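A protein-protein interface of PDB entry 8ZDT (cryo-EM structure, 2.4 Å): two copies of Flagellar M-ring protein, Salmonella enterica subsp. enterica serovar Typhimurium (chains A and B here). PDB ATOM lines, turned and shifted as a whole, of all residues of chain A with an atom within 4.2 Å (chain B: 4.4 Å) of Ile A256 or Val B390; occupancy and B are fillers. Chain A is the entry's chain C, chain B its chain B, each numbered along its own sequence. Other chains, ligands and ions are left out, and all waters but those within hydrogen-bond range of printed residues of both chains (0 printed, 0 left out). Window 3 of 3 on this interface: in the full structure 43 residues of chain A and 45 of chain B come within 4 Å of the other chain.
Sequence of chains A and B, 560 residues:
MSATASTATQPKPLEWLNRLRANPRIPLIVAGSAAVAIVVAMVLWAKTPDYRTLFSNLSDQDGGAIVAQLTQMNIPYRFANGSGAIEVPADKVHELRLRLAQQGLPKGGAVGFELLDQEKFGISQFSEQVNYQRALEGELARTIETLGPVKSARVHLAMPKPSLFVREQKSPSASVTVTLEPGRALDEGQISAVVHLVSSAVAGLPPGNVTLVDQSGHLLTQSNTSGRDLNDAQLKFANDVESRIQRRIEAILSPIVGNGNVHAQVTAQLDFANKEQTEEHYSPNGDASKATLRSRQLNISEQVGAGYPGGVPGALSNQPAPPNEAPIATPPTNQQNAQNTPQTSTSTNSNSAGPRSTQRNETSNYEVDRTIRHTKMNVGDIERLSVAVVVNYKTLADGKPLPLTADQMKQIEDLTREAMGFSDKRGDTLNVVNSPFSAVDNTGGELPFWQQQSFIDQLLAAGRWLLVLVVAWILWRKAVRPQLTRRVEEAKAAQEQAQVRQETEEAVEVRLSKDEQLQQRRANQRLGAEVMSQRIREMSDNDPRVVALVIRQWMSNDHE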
ATOM      1  N   LEU A 253     -15.448 -28.621 -23.385  1.00  0.00           N
ATOM      2  CA  LEU A 253     -16.283 -28.922 -22.226  1.00  0.00           C
ATOM      3  C   LEU A 253     -15.532 -29.563 -21.062  1.00  0.00           C
ATOM      4  O   LEU A 253     -16.026 -29.508 -19.930  1.00  0.00           O
ATOM      5  CB  LEU A 253     -17.443 -29.838 -22.628  1.00  0.00           C
ATOM      6  CG  LEU A 253     -18.636 -29.178 -23.320  1.00  0.00           C
ATOM      7  CD1 LEU A 253     -19.821 -30.128 -23.358  1.00  0.00           C
ATOM      8  CD2 LEU A 253     -19.010 -27.882 -22.619  1.00  0.00           C
ATOM      9  N   SER A 254     -14.367 -30.166 -21.303  1.00  0.00           N
ATOM     10  CA  SER A 254     -13.673 -30.885 -20.234  1.00  0.00           C
ATOM     11  C   SER A 254     -13.284 -30.013 -19.044  1.00  0.00           C
ATOM     12  O   SER A 254     -13.506 -30.445 -17.899  1.00  0.00           O
ATOM     13  CB  SER A 254     -12.449 -31.600 -20.815  1.00  0.00           C
ATOM     14  OG  SER A 254     -12.787 -32.899 -21.270  1.00  0.00           O
ATOM     15  N   PRO A 255     -12.704 -28.817 -19.213  1.00  0.00           N
ATOM     16  CA  PRO A 255     -12.227 -28.067 -18.037  1.00  0.00           C
ATOM     17  C   PRO A 255     -13.310 -27.701 -17.035  1.00  0.00           C
ATOM     18  O   PRO A 255     -12.990 -27.483 -15.861  1.00  0.00           O
ATOM     19  CB  PRO A 255     -11.601 -26.807 -18.660  1.00  0.00           C
ATOM     20  CG  PRO A 255     -12.218 -26.728 -20.028  1.00  0.00           C
ATOM     21  CD  PRO A 255     -12.258 -28.154 -20.450  1.00  0.00           C
ATOM     22  N   ILE A 256     -14.574 -27.623 -17.447  1.00  0.00           N
ATOM     23  CA  ILE A 256     -15.633 -27.149 -16.563  1.00  0.00           C
ATOM     24  C   ILE A 256     -16.187 -28.291 -15.719  1.00  0.00           C
ATOM     25  O   ILE A 256     -16.207 -28.210 -14.485  1.00  0.00           O
ATOM     26  CB  ILE A 256     -16.759 -26.470 -17.363  1.00  0.00           C
ATOM     27  CG1 ILE A 256     -16.276 -25.134 -17.930  1.00  0.00           C
ATOM     28  CG2 ILE A 256     -17.987 -26.270 -16.488  1.00  0.00           C
ATOM     29  CD1 ILE A 256     -17.393 -24.233 -18.412  1.00  0.00           C
ATOM     30  N   VAL A 257     -16.645 -29.360 -16.371  1.00  0.00           N
ATOM     31  CA  VAL A 257     -17.335 -30.419 -15.641  1.00  0.00           C
ATOM     32  C   VAL A 257     -16.369 -31.497 -15.157  1.00  0.00           C
ATOM     33  O   VAL A 257     -16.650 -32.183 -14.168  1.00  0.00           O
ATOM     34  CB  VAL A 257     -18.455 -31.020 -16.509  1.00  0.00           C
ATOM     35  CG1 VAL A 257     -19.372 -29.923 -17.022  1.00  0.00           C
ATOM     36  CG2 VAL A 257     -17.868 -31.810 -17.670  1.00  0.00           C
ATOM     37  N   GLY A 258     -15.232 -31.668 -15.825  1.00  0.00           N
ATOM     38  CA  GLY A 258     -14.302 -32.720 -15.463  1.00  0.00           C
ATOM     39  C   GLY A 258     -13.759 -33.460 -16.667  1.00  0.00           C
ATOM     40  O   GLY A 258     -14.268 -33.304 -17.781  1.00  0.00           O
ATOM     41  N   LEU A 415     -21.781 -23.002 -24.870  1.00  0.00           N
ATOM     42  CA  LEU A 415     -20.443 -23.412 -25.286  1.00  0.00           C
ATOM     43  C   LEU A 415     -20.506 -24.479 -26.372  1.00  0.00           C
ATOM     44  O   LEU A 415     -19.733 -24.438 -27.336  1.00  0.00           O
ATOM     45  CB  LEU A 415     -19.652 -23.916 -24.080  1.00  0.00           C
ATOM     46  CG  LEU A 415     -19.228 -22.850 -23.068  1.00  0.00           C
ATOM     47  CD1 LEU A 415     -18.504 -23.482 -21.893  1.00  0.00           C
ATOM     48  CD2 LEU A 415     -18.358 -21.795 -23.732  1.00  0.00           C
ATOM     49  N   ASN B 261      -4.938 -20.257 -17.023  1.00  0.00           N
ATOM     50  CA  ASN B 261      -6.264 -19.954 -16.497  1.00  0.00           C
ATOM     51  C   ASN B 261      -7.235 -19.547 -17.602  1.00  0.00           C
ATOM     52  O   ASN B 261      -8.222 -18.857 -17.342  1.00  0.00           O
ATOM     53  CB  ASN B 261      -6.184 -18.861 -15.432  1.00  0.00           C
ATOM     54  CG  ASN B 261      -5.338 -19.265 -14.239  1.00  0.00           C
ATOM     55  OD1 ASN B 261      -5.863 -19.649 -13.195  1.00  0.00           O
ATOM     56  ND2 ASN B 261      -4.022 -19.174 -14.387  1.00  0.00           N
ATOM     57  N   VAL B 262      -6.975 -19.968 -18.837  1.00  0.00           N
ATOM     58  CA  VAL B 262      -7.828 -19.606 -19.965  1.00  0.00           C
ATOM     59  C   VAL B 262      -7.703 -20.676 -21.042  1.00  0.00           C
ATOM     60  O   VAL B 262      -6.617 -21.213 -21.281  1.00  0.00           O
ATOM     61  CB  VAL B 262      -7.470 -18.202 -20.507  1.00  0.00           C
ATOM     62  CG1 VAL B 262      -6.014 -18.148 -20.954  1.00  0.00           C
ATOM     63  CG2 VAL B 262      -8.403 -17.803 -21.643  1.00  0.00           C
ATOM     64  N   HIS B 263      -8.829 -20.998 -21.678  1.00  0.00           N
ATOM     65  CA  HIS B 263      -8.869 -21.917 -22.806  1.00  0.00           C
ATOM     66  C   HIS B 263      -9.798 -21.355 -23.871  1.00  0.00           C
ATOM     67  O   HIS B 263     -10.782 -20.679 -23.561  1.00  0.00           O
ATOM     68  CB  HIS B 263      -9.338 -23.319 -22.392  1.00  0.00           C
ATOM     69  CG  HIS B 263      -8.562 -23.908 -21.257  1.00  0.00           C
ATOM     70  ND1 HIS B 263      -7.546 -24.820 -21.444  1.00  0.00           N
ATOM     71  CD2 HIS B 263      -8.657 -23.720 -19.919  1.00  0.00           C
ATOM     72  CE1 HIS B 263      -7.047 -25.166 -20.271  1.00  0.00           C
ATOM     73  NE2 HIS B 263      -7.703 -24.513 -19.330  1.00  0.00           N
ATOM     74  N   VAL B 389     -14.777 -19.124 -25.184  1.00  0.00           N
ATOM     75  CA  VAL B 389     -13.682 -18.932 -24.238  1.00  0.00           C
ATOM     76  C   VAL B 389     -14.185 -19.223 -22.830  1.00  0.00           C
ATOM     77  O   VAL B 389     -15.317 -18.870 -22.480  1.00  0.00           O
ATOM     78  CB  VAL B 389     -13.101 -17.502 -24.315  1.00  0.00           C
ATOM     79  CG1 VAL B 389     -11.792 -17.414 -23.545  1.00  0.00           C
ATOM     80  CG2 VAL B 389     -12.897 -17.078 -25.761  1.00  0.00           C
ATOM     81  N   VAL B 390     -13.345 -19.871 -22.024  1.00  0.00           N
ATOM     82  CA  VAL B 390     -13.634 -20.144 -20.619  1.00  0.00           C
ATOM     83  C   VAL B 390     -12.537 -19.515 -19.770  1.00  0.00           C
ATOM     84  O   VAL B 390     -11.347 -19.692 -20.053  1.00  0.00           O
ATOM     85  CB  VAL B 390     -13.748 -21.655 -20.338  1.00  0.00           C
ATOM     86  CG1 VAL B 390     -15.124 -22.163 -20.734  1.00  0.00           C
ATOM     87  CG2 VAL B 390     -12.661 -22.424 -21.070  1.00  0.00           C
ATOM     88  N   VAL B 391     -12.939 -18.783 -18.733  1.00  0.00           N
ATOM     89  CA  VAL B 391     -12.022 -18.050 -17.867  1.00  0.00           C
ATOM     90  C   VAL B 391     -12.119 -18.618 -16.458  1.00  0.00           C
ATOM     91  O   VAL B 391     -13.221 -18.757 -15.913  1.00  0.00           O
ATOM     92  CB  VAL B 391     -12.323 -16.539 -17.869  1.00  0.00           C
ATOM     93  CG1 VAL B 391     -11.344 -15.799 -16.972  1.00  0.00           C
ATOM     94  CG2 VAL B 391     -12.271 -15.992 -19.285  1.00  0.00           C
ATOM     95  N   ASN B 392     -10.969 -18.940 -15.871  1.00  0.00           N
ATOM     96  CA  ASN B 392     -10.922 -19.523 -14.539  1.00  0.00           C
ATOM     97  C   ASN B 392     -11.221 -18.476 -13.468  1.00  0.00           C
ATOM     98  O   ASN B 392     -11.031 -17.272 -13.661  1.00  0.00           O
ATOM     99  CB  ASN B 392      -9.552 -20.153 -14.279  1.00  0.00           C
ATOM    100  CG  ASN B 392      -9.549 -21.072 -13.072  1.00  0.00           C
ATOM    101  OD1 ASN B 392     -10.584 -21.300 -12.446  1.00  0.00           O
ATOM    102  ND2 ASN B 392      -8.379 -21.606 -12.739  1.00  0.00           N
ATOM    103  N   VAL B 433     -17.319 -17.359 -21.016  1.00  0.00           N
ATOM    104  CA  VAL B 433     -17.946 -17.859 -19.797  1.00  0.00           C
ATOM    105  C   VAL B 433     -16.912 -17.867 -18.679  1.00  0.00           C
ATOM    106  O   VAL B 433     -15.810 -18.398 -18.851  1.00  0.00           O
ATOM    107  CB  VAL B 433     -18.533 -19.270 -20.000  1.00  0.00           C
ATOM    108  CG1 VAL B 433     -18.852 -19.916 -18.662  1.00  0.00           C
ATOM    109  CG2 VAL B 433     -19.774 -19.206 -20.872  1.00  0.00           C
ATOM    110  N   SER B 435     -16.185 -19.351 -15.075  1.00  0.00           N
ATOM    111  CA  SER B 435     -16.617 -20.448 -14.222  1.00  0.00           C
ATOM    112  C   SER B 435     -15.399 -21.070 -13.562  1.00  0.00           C
ATOM    113  O   SER B 435     -14.314 -21.081 -14.156  1.00  0.00           O
ATOM    114  CB  SER B 435     -17.386 -21.510 -15.023  1.00  0.00           C
ATOM    115  OG  SER B 435     -17.197 -22.803 -14.477  1.00  0.00           O
ATOM    116  N   PHE B 437     -12.663 -23.761 -12.377  1.00  0.00           N
ATOM    117  CA  PHE B 437     -12.090 -24.918 -13.050  1.00  0.00           C
ATOM    118  C   PHE B 437     -12.030 -26.102 -12.093  1.00  0.00           C
ATOM    119  O   PHE B 437     -11.784 -25.937 -10.896  1.00  0.00           O
ATOM    120  CB  PHE B 437     -10.689 -24.603 -13.577  1.00  0.00           C
ATOM    121  CG  PHE B 437     -10.681 -23.797 -14.849  1.00  0.00           C
ATOM    122  CD1 PHE B 437     -11.853 -23.275 -15.367  1.00  0.00           C
ATOM    123  CD2 PHE B 437      -9.496 -23.566 -15.526  1.00  0.00           C
ATOM    124  CE1 PHE B 437     -11.844 -22.534 -16.533  1.00  0.00           C
ATOM    125  CE2 PHE B 437      -9.479 -22.828 -16.693  1.00  0.00           C
ATOM    126  CZ  PHE B 437     -10.655 -22.312 -17.197  1.00  0.00           C
ATOM    127  N   SER B 438     -12.255 -27.296 -12.631  1.00  0.00           N
ATOM    128  CA  SER B 438     -12.221 -28.513 -11.829  1.00  0.00           C
ATOM    129  C   SER B 438     -10.786 -28.983 -11.608  1.00  0.00           C
ATOM    130  O   SER B 438     -10.390 -29.290 -10.484  1.00  0.00           O
ATOM    131  CB  SER B 438     -13.039 -29.621 -12.497  1.00  0.00           C
ATOM    132  OG  SER B 438     -12.284 -30.279 -13.498  1.00  0.00           O
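The backbone carbonyl oxygen of Pro A255 lies within hydrogen-bond range of the backbone NH of Ser B438 (3.3 Å).
Of the printed residues of chain B, Ile A256 touches Val B390 (3.9 Å) and Ser B438 (3.997 Å). Of chain A, only Ile A256 (3.9 Å) and Leu A415 (3.8 Å) come within 4 Å of Val B390. Printed residues of chain B within 4 Å of Leu A415: Val B390 (3.8 Å). Of the printed residues of chain A, Ser B438 touches Pro A255, Ile A256 and Gly A258. Of the printed residues of chain B, Gly A258 touches Ser B438. Printed residues of chain A within 4 Å of Phe B437: Pro A255 (3.9 Å). Printed residues of chain B within 4 Å of Pro A255: Phe B437 (3.9 Å) and Ser B438 (3.3 Å). Ser B435 touches none of the printed residues of chain A. The nearest printed residue of chain B that does not touch Gly A258 is Phe B437 (7.4 Å).
The backbone NH of Val B390 lies within hydrogen-bond range of the backbone carbonyl oxygen of His B263 (3.1 Å). The backbone NH (N) of Phe B437 lies within hydrogen-bond range of the side-chain amide oxygen (OD1) of Asn B392, at 3.2 Å.
No position is printed for both chains.
Phe B437 touches Pro A255 (CA to O, 3.9 Å). Ile A256 touches Val B390. Ser B438 touches Ile A256. Ser B438 touches Gly A258. CD1 of Leu A415 touches CG1 of Val B390, 3.8 Å away.
Of the 11 printed residues of chain B, 3 touch a printed residue of chain A.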
